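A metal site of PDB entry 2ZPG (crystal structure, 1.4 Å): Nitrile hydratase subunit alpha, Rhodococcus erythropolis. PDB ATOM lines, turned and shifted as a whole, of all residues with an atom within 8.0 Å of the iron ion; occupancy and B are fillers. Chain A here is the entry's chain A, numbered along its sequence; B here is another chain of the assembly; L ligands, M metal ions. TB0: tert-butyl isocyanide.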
ATOM      1  N   GLN A  90     -11.924  23.748  13.359  1.00  0.00           N
ATOM      2  CA  GLN A  90     -12.289  22.340  13.551  1.00  0.00           C
ATOM      3  C   GLN A  90     -13.781  22.176  13.876  1.00  0.00           C
ATOM      4  O   GLN A  90     -14.194  21.235  14.545  1.00  0.00           O
ATOM      5  CB  GLN A  90     -11.407  21.667  14.607  1.00  0.00           C
ATOM      6  CG  GLN A  90      -9.951  21.532  14.159  1.00  0.00           C
ATOM      7  CD  GLN A  90      -9.832  20.706  12.902  1.00  0.00           C
ATOM      8  OE1 GLN A  90     -10.287  19.561  12.888  1.00  0.00           O
ATOM      9  NE2 GLN A  90      -9.260  21.262  11.850  1.00  0.00           N
ATOM     10  N   VAL A 108     -15.778   8.942  16.756  1.00  0.00           N
ATOM     11  CA  VAL A 108     -14.341   8.713  16.967  1.00  0.00           C
ATOM     12  C   VAL A 108     -13.563   9.378  15.826  1.00  0.00           C
ATOM     13  O   VAL A 108     -14.145   9.731  14.799  1.00  0.00           O
ATOM     14  CB  VAL A 108     -14.027   7.188  17.001  1.00  0.00           C
ATOM     15  CG1 VAL A 108     -14.345   6.528  15.657  1.00  0.00           C
ATOM     16  CG2 VAL A 108     -12.571   6.920  17.402  1.00  0.00           C
ATOM     17  N   CYS A 109     -12.252   9.569  16.016  1.00  0.00           N
ATOM     18  CA  CYS A 109     -11.362   9.813  14.894  1.00  0.00           C
ATOM     19  C   CYS A 109     -10.301   8.726  14.956  1.00  0.00           C
ATOM     20  O   CYS A 109      -9.306   8.849  15.687  1.00  0.00           O
ATOM     21  CB  CYS A 109     -10.710  11.182  14.997  1.00  0.00           C
ATOM     22  SG  CYS A 109      -9.480  11.479  13.658  1.00  0.00           S
ATOM     23  N   SER A 110     -10.482   7.658  14.188  1.00  0.00           N
ATOM     24  CA  SER A 110      -9.560   6.530  14.311  1.00  0.00           C
ATOM     25  C   SER A 110      -8.149   6.869  13.834  1.00  0.00           C
ATOM     26  O   SER A 110      -7.176   6.279  14.311  1.00  0.00           O
ATOM     27  CB  SER A 110     -10.094   5.295  13.586  1.00  0.00           C
ATOM     28  OG  SER A 110     -10.051   5.461  12.176  1.00  0.00           O
ATOM     29  N   LEU A 111      -8.033   7.802  12.885  1.00  0.00           N
ATOM     30  CA  LEU A 111      -6.755   8.126  12.266  1.00  0.00           C
ATOM     31  C   LEU A 111      -5.940   9.116  13.059  1.00  0.00           C
ATOM     32  O   LEU A 111      -4.753   9.341  12.784  1.00  0.00           O
ATOM     33  CB  LEU A 111      -6.960   8.641  10.839  1.00  0.00           C
ATOM     34  CG  LEU A 111      -7.553   7.599   9.884  1.00  0.00           C
ATOM     35  CD1 LEU A 111      -7.987   8.270   8.584  1.00  0.00           C
ATOM     36  CD2 LEU A 111      -6.540   6.491   9.615  1.00  0.00           C
ATOM     37  N   CSD A 112      -6.594   9.936  14.122  1.00  0.00           N
ATOM     38  CA  CSD A 112      -5.854  10.955  14.857  1.00  0.00           C
ATOM     39  CB  CSD A 112      -5.389  12.128  13.961  1.00  0.00           C
ATOM     40  SG  CSD A 112      -6.614  12.824  12.879  1.00  0.00           S
ATOM     41  C   CSD A 112      -6.691  11.417  16.021  1.00  0.00           C
ATOM     42  O   CSD A 112      -6.623  10.850  17.107  1.00  0.00           O
ATOM     43  OD1 CSD A 112      -5.859  13.972  12.227  1.00  0.00           O
ATOM     44  OD2 CSD A 112      -6.934  11.798  11.829  1.00  0.00           O
ATOM     45  N   SER A 113      -7.630  12.590  15.881  1.00  0.00           N
ATOM     46  CA  SER A 113      -8.293  13.064  17.141  1.00  0.00           C
ATOM     47  C   SER A 113      -9.429  14.006  16.794  1.00  0.00           C
ATOM     48  O   SER A 113     -10.093  14.557  17.659  1.00  0.00           O
ATOM     49  CB  SER A 113      -7.304  13.792  18.031  1.00  0.00           C
ATOM     50  OG  SER A 113      -6.833  14.980  17.393  1.00  0.00           O
ATOM     51  N   CSO A 114      -9.719  14.065  15.319  1.00  0.00           N
ATOM     52  CA  CSO A 114     -10.686  15.010  14.792  1.00  0.00           C
ATOM     53  CB  CSO A 114     -10.941  14.712  13.321  1.00  0.00           C
ATOM     54  SG  CSO A 114      -9.380  14.477  12.530  1.00  0.00           S
ATOM     55  C   CSO A 114     -11.997  14.924  15.560  1.00  0.00           C
ATOM     56  O   CSO A 114     -12.575  13.912  15.959  1.00  0.00           O
ATOM     57  OD  CSO A 114      -8.945  15.938  12.233  1.00  0.00           O
ATOM     58  N   THR A 115     -12.392  16.271  16.041  1.00  0.00           N
ATOM     59  CA  THR A 115     -13.407  16.590  17.069  1.00  0.00           C
ATOM     60  C   THR A 115     -13.948  17.955  16.703  1.00  0.00           C
ATOM     61  O   THR A 115     -13.167  18.822  16.276  1.00  0.00           O
ATOM     62  CB  THR A 115     -12.757  16.656  18.470  1.00  0.00           C
ATOM     63  OG1 THR A 115     -12.358  15.331  18.856  1.00  0.00           O
ATOM     64  CG2 THR A 115     -13.708  17.230  19.520  1.00  0.00           C
ATOM     65  N   TRP A 117     -14.249  20.867  17.841  1.00  0.00           N
ATOM     66  CA  TRP A 117     -13.690  21.653  18.951  1.00  0.00           C
ATOM     67  C   TRP A 117     -14.580  22.737  19.562  1.00  0.00           C
ATOM     68  O   TRP A 117     -14.683  22.809  20.779  1.00  0.00           O
ATOM     69  CB  TRP A 117     -12.371  22.321  18.554  1.00  0.00           C
ATOM     70  CG  TRP A 117     -11.187  21.443  18.338  1.00  0.00           C
ATOM     71  CD1 TRP A 117     -11.043  20.124  18.632  1.00  0.00           C
ATOM     72  CD2 TRP A 117      -9.929  21.879  17.799  1.00  0.00           C
ATOM     73  NE1 TRP A 117      -9.777  19.696  18.292  1.00  0.00           N
ATOM     74  CE2 TRP A 117      -9.071  20.753  17.784  1.00  0.00           C
ATOM     75  CE3 TRP A 117      -9.459  23.106  17.336  1.00  0.00           C
ATOM     76  CZ2 TRP A 117      -7.756  20.834  17.312  1.00  0.00           C
ATOM     77  CZ3 TRP A 117      -8.164  23.182  16.855  1.00  0.00           C
ATOM     78  CH2 TRP A 117      -7.321  22.050  16.855  1.00  0.00           C
ATOM     79  N   PRO A 123     -10.546  17.462  22.395  1.00  0.00           N
ATOM     80  CA  PRO A 123     -10.793  16.094  22.838  1.00  0.00           C
ATOM     81  C   PRO A 123     -10.052  15.742  24.114  1.00  0.00           C
ATOM     82  O   PRO A 123      -8.946  16.228  24.341  1.00  0.00           O
ATOM     83  CB  PRO A 123     -10.273  15.240  21.670  1.00  0.00           C
ATOM     84  CG  PRO A 123      -9.312  16.116  20.958  1.00  0.00           C
ATOM     85  CD  PRO A 123      -9.893  17.506  21.074  1.00  0.00           C
ATOM     86  N   TYR A 127     -10.134   9.973  24.415  1.00  0.00           N
ATOM     87  CA  TYR A 127     -10.678   9.942  23.063  1.00  0.00           C
ATOM     88  C   TYR A 127      -9.564   9.779  22.041  1.00  0.00           C
ATOM     89  O   TYR A 127      -9.762   9.200  20.973  1.00  0.00           O
ATOM     90  CB  TYR A 127     -11.480  11.208  22.828  1.00  0.00           C
ATOM     91  CG  TYR A 127     -12.065  11.407  21.445  1.00  0.00           C
ATOM     92  CD1 TYR A 127     -11.357  12.059  20.434  1.00  0.00           C
ATOM     93  CD2 TYR A 127     -13.380  10.987  21.174  1.00  0.00           C
ATOM     94  CE1 TYR A 127     -11.923  12.275  19.191  1.00  0.00           C
ATOM     95  CE2 TYR A 127     -13.955  11.214  19.934  1.00  0.00           C
ATOM     96  CZ  TYR A 127     -13.220  11.864  18.941  1.00  0.00           C
ATOM     97  OH  TYR A 127     -13.777  12.124  17.700  1.00  0.00           O
ATOM     98  N   LYS A 128      -8.400  10.349  22.377  1.00  0.00           N
ATOM     99  CA  LYS A 128      -7.209  10.276  21.540  1.00  0.00           C
ATOM    100  C   LYS A 128      -6.406   9.010  21.775  1.00  0.00           C
ATOM    101  O   LYS A 128      -5.403   8.788  21.096  1.00  0.00           O
ATOM    102  CB  LYS A 128      -6.318  11.497  21.816  1.00  0.00           C
ATOM    103  CG  LYS A 128      -7.003  12.802  21.457  1.00  0.00           C
ATOM    104  CD  LYS A 128      -6.234  14.021  21.874  1.00  0.00           C
ATOM    105  CE  LYS A 128      -6.398  14.347  23.351  1.00  0.00           C
ATOM    106  NZ  LYS A 128      -5.849  15.695  23.694  1.00  0.00           N
ATOM    107  N   ARG A 133      -9.316   4.575  19.690  1.00  0.00           N
ATOM    108  CA  ARG A 133      -9.147   4.654  18.251  1.00  0.00           C
ATOM    109  C   ARG A 133      -9.164   3.284  17.562  1.00  0.00           C
ATOM    110  O   ARG A 133      -9.658   3.145  16.441  1.00  0.00           O
ATOM    111  CB  ARG A 133      -7.837   5.394  17.942  1.00  0.00           C
ATOM    112  CG  ARG A 133      -7.932   6.898  18.209  1.00  0.00           C
ATOM    113  CD  ARG A 133      -6.604   7.625  18.012  1.00  0.00           C
ATOM    114  NE  ARG A 133      -6.044   7.300  16.710  1.00  0.00           N
ATOM    115  CZ  ARG A 133      -4.762   7.423  16.370  1.00  0.00           C
ATOM    116  NH1 ARG A 133      -3.876   7.922  17.231  1.00  0.00           N
ATOM    117  NH2 ARG A 133      -4.357   7.036  15.164  1.00  0.00           N
ATOM    118  N   ASP A 161     -16.788   7.667  12.074  1.00  0.00           N
ATOM    119  CA  ASP A 161     -15.343   7.882  12.064  1.00  0.00           C
ATOM    120  C   ASP A 161     -15.082   9.204  11.329  1.00  0.00           C
ATOM    121  O   ASP A 161     -15.407   9.354  10.158  1.00  0.00           O
ATOM    122  CB  ASP A 161     -14.644   6.715  11.371  1.00  0.00           C
ATOM    123  CG  ASP A 161     -13.153   6.646  11.665  1.00  0.00           C
ATOM    124  OD1 ASP A 161     -12.607   7.599  12.275  1.00  0.00           O
ATOM    125  OD2 ASP A 161     -12.545   5.624  11.288  1.00  0.00           O
ATOM    126  N   THR A 162     -14.499  10.157  12.057  1.00  0.00           N
ATOM    127  CA  THR A 162     -14.297  11.508  11.575  1.00  0.00           C
ATOM    128  C   THR A 162     -13.050  11.557  10.712  1.00  0.00           C
ATOM    129  O   THR A 162     -11.960  11.853  11.189  1.00  0.00           O
ATOM    130  CB  THR A 162     -14.182  12.495  12.766  1.00  0.00           C
ATOM    131  OG1 THR A 162     -15.301  12.294  13.653  1.00  0.00           O
ATOM    132  CG2 THR A 162     -14.194  13.918  12.283  1.00  0.00           C
ATOM    133  N   THR A 163     -13.203  11.247   9.433  1.00  0.00           N
ATOM    134  CA  THR A 163     -12.088  11.034   8.511  1.00  0.00           C
ATOM    135  C   THR A 163     -11.868  12.174   7.531  1.00  0.00           C
ATOM    136  O   THR A 163     -10.874  12.177   6.798  1.00  0.00           O
ATOM    137  CB  THR A 163     -12.301   9.726   7.729  1.00  0.00           C
ATOM    138  OG1 THR A 163     -13.651   9.690   7.226  1.00  0.00           O
ATOM    139  CG2 THR A 163     -12.081   8.506   8.610  1.00  0.00           C
ATOM    140  N   ALA A 164     -12.783  13.140   7.493  1.00  0.00           N
ATOM    141  CA  ALA A 164     -12.628  14.273   6.596  1.00  0.00           C
ATOM    142  C   ALA A 164     -12.924  15.582   7.321  1.00  0.00           C
ATOM    143  O   ALA A 164     -12.399  15.789   8.417  1.00  0.00           O
ATOM    144  CB  ALA A 164     -13.457  14.086   5.307  1.00  0.00           C
ATOM    145  N   ARG A 167     -17.639  17.595  11.044  1.00  0.00           N
ATOM    146  CA  ARG A 167     -17.400  17.535  12.466  1.00  0.00           C
ATOM    147  C   ARG A 167     -18.738  17.254  13.130  1.00  0.00           C
ATOM    148  O   ARG A 167     -19.726  17.941  12.844  1.00  0.00           O
ATOM    149  CB  ARG A 167     -16.754  18.833  12.952  1.00  0.00           C
ATOM    150  CG  ARG A 167     -15.346  19.071  12.395  1.00  0.00           C
ATOM    151  CD  ARG A 167     -14.324  18.155  13.056  1.00  0.00           C
ATOM    152  NE  ARG A 167     -13.007  18.287  12.454  1.00  0.00           N
ATOM    153  CZ  ARG A 167     -12.624  17.648  11.352  1.00  0.00           C
ATOM    154  NH1 ARG A 167     -13.445  16.812  10.733  1.00  0.00           N
ATOM    155  NH2 ARG A 167     -11.398  17.845  10.866  1.00  0.00           N
ATOM    156  N   TYR B  37      -0.834  23.014  18.964  1.00  0.00           N
ATOM    157  CA  TYR B  37      -1.957  23.518  18.171  1.00  0.00           C
ATOM    158  C   TYR B  37      -1.792  24.988  17.794  1.00  0.00           C
ATOM    159  O   TYR B  37      -2.073  25.384  16.652  1.00  0.00           O
ATOM    160  CB  TYR B  37      -3.290  23.344  18.898  1.00  0.00           C
ATOM    161  CG  TYR B  37      -3.871  21.950  19.017  1.00  0.00           C
ATOM    162  CD1 TYR B  37      -3.375  20.848  18.303  1.00  0.00           C
ATOM    163  CD2 TYR B  37      -4.995  21.743  19.829  1.00  0.00           C
ATOM    164  CE1 TYR B  37      -3.969  19.580  18.424  1.00  0.00           C
ATOM    165  CE2 TYR B  37      -5.578  20.510  19.954  1.00  0.00           C
ATOM    166  CZ  TYR B  37      -5.074  19.437  19.262  1.00  0.00           C
ATOM    167  OH  TYR B  37      -5.711  18.220  19.413  1.00  0.00           O
ATOM    168  N   ARG B  56      -1.227  16.422   9.554  1.00  0.00           N
ATOM    169  CA  ARG B  56      -1.636  15.029   9.735  1.00  0.00           C
ATOM    170  C   ARG B  56      -0.600  14.075   9.169  1.00  0.00           C
ATOM    171  O   ARG B  56      -0.188  13.116   9.818  1.00  0.00           O
ATOM    172  CB  ARG B  56      -2.987  14.748   9.073  1.00  0.00           C
ATOM    173  CG  ARG B  56      -4.143  15.497   9.683  1.00  0.00           C
ATOM    174  CD  ARG B  56      -5.487  14.903   9.247  1.00  0.00           C
ATOM    175  NE  ARG B  56      -6.543  15.640   9.927  1.00  0.00           N
ATOM    176  CZ  ARG B  56      -7.109  16.741   9.442  1.00  0.00           C
ATOM    177  NH1 ARG B  56      -6.748  17.212   8.246  1.00  0.00           N
ATOM    178  NH2 ARG B  56      -8.050  17.379  10.150  1.00  0.00           N
ATOM    179  N   TYR B  72       0.075  12.007  22.708  1.00  0.00           N
ATOM    180  CA  TYR B  72      -0.581  12.793  21.692  1.00  0.00           C
ATOM    181  C   TYR B  72       0.012  14.198  21.450  1.00  0.00           C
ATOM    182  O   TYR B  72       0.423  14.518  20.327  1.00  0.00           O
ATOM    183  CB  TYR B  72      -2.076  12.918  22.055  1.00  0.00           C
ATOM    184  CG  TYR B  72      -2.814  13.775  21.078  1.00  0.00           C
ATOM    185  CD1 TYR B  72      -3.320  13.237  19.908  1.00  0.00           C
ATOM    186  CD2 TYR B  72      -2.963  15.156  21.304  1.00  0.00           C
ATOM    187  CE1 TYR B  72      -3.971  14.022  18.982  1.00  0.00           C
ATOM    188  CE2 TYR B  72      -3.615  15.960  20.372  1.00  0.00           C
ATOM    189  CZ  TYR B  72      -4.118  15.374  19.218  1.00  0.00           C
ATOM    190  OH  TYR B  72      -4.773  16.138  18.291  1.00  0.00           O
ATOM    191  N   TYR B  76       2.476  16.142  18.008  1.00  0.00           N
ATOM    192  CA  TYR B  76       2.270  17.371  17.246  1.00  0.00           C
ATOM    193  C   TYR B  76       3.411  18.367  17.406  1.00  0.00           C
ATOM    194  O   TYR B  76       3.702  19.113  16.469  1.00  0.00           O
ATOM    195  CB  TYR B  76       0.880  17.976  17.509  1.00  0.00           C
ATOM    196  CG  TYR B  76      -0.152  17.033  16.955  1.00  0.00           C
ATOM    197  CD1 TYR B  76      -0.605  17.127  15.642  1.00  0.00           C
ATOM    198  CD2 TYR B  76      -0.575  15.953  17.714  1.00  0.00           C
ATOM    199  CE1 TYR B  76      -1.520  16.192  15.124  1.00  0.00           C
ATOM    200  CE2 TYR B  76      -1.458  15.029  17.220  1.00  0.00           C
ATOM    201  CZ  TYR B  76      -1.939  15.150  15.931  1.00  0.00           C
ATOM    202  OH  TYR B  76      -2.817  14.191  15.487  1.00  0.00           O
ATOM    203  N   ARG B 141      -7.035   9.840   3.405  1.00  0.00           N
ATOM    204  CA  ARG B 141      -8.020   9.880   4.478  1.00  0.00           C
ATOM    205  C   ARG B 141      -9.020   8.752   4.337  1.00  0.00           C
ATOM    206  O   ARG B 141     -10.235   8.899   4.529  1.00  0.00           O
ATOM    207  CB  ARG B 141      -8.715  11.247   4.548  1.00  0.00           C
ATOM    208  CG  ARG B 141      -7.772  12.353   4.975  1.00  0.00           C
ATOM    209  CD  ARG B 141      -7.096  12.026   6.308  1.00  0.00           C
ATOM    210  NE  ARG B 141      -8.053  12.109   7.408  1.00  0.00           N
ATOM    211  CZ  ARG B 141      -7.730  11.932   8.686  1.00  0.00           C
ATOM    212  NH1 ARG B 141      -6.488  11.595   9.019  1.00  0.00           N
ATOM    213  NH2 ARG B 141      -8.647  12.096   9.614  1.00  0.00           N
HETATM  214  C   TB0 L   1      -7.167  15.146  14.508  1.00  0.00           C
HETATM  215  N   TB0 L   1      -6.707  16.182  14.386  1.00  0.00           N
HETATM  216  C2  TB0 L   1      -6.118  17.466  14.222  1.00  0.00           C
HETATM  217  C4  TB0 L   1      -5.345  17.808  15.481  1.00  0.00           C
HETATM  218  C3  TB0 L   1      -7.254  18.440  13.969  1.00  0.00           C
HETATM  219  C1  TB0 L   1      -5.177  17.422  13.023  1.00  0.00           C
HETATM  220 FE    FE M   1      -8.250  13.431  14.152  1.00  0.00          FE
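OD of CSO 114 is in hydrogen-bond range of the guanidinium group of Arg 56 of chain B (2.7 Å). OD of CSO 114 is in hydrogen-bond range of NH2 of Arg 167 (3.4 Å). O of CSO 114 lies within hydrogen-bond range of OH of Tyr 127. The backbone carbonyl oxygen of Ser 113 lies within hydrogen-bond range of the side-chain hydroxyl of Thr 115. OG of Ser 113 lies within hydrogen-bond range of OH of Tyr 72 of chain B (2.5 Å). OD2 of CSD 112 is in salt-bridge range of the guanidinium group (NH2) of Arg 141 of chain B (2.8 Å). O of Thr 162 lies close to SG of Cys 109 (3.5 Å). N of Cys 109 lies within hydrogen-bond range of OH of Tyr 127 (3.4 Å).
Of the 24 residues printed, 4 come within 4 Å of the iron ion. Along chain A the residues within 4 Å of the iron ion span positions 109 to 114. The nearest printed residue that does not touch the iron ion is Arg 141 of chain B (4.7 Å).
The iron ion is bound by N of CSO 114 (2.0 Å), the backbone nitrogen of Ser 113 (2.0 Å), SG of CSD 112 (2.2 Å), SG of CSO 114 (2.2 Å) and the side-chain sulfur of Cys 109 (2.4 Å).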
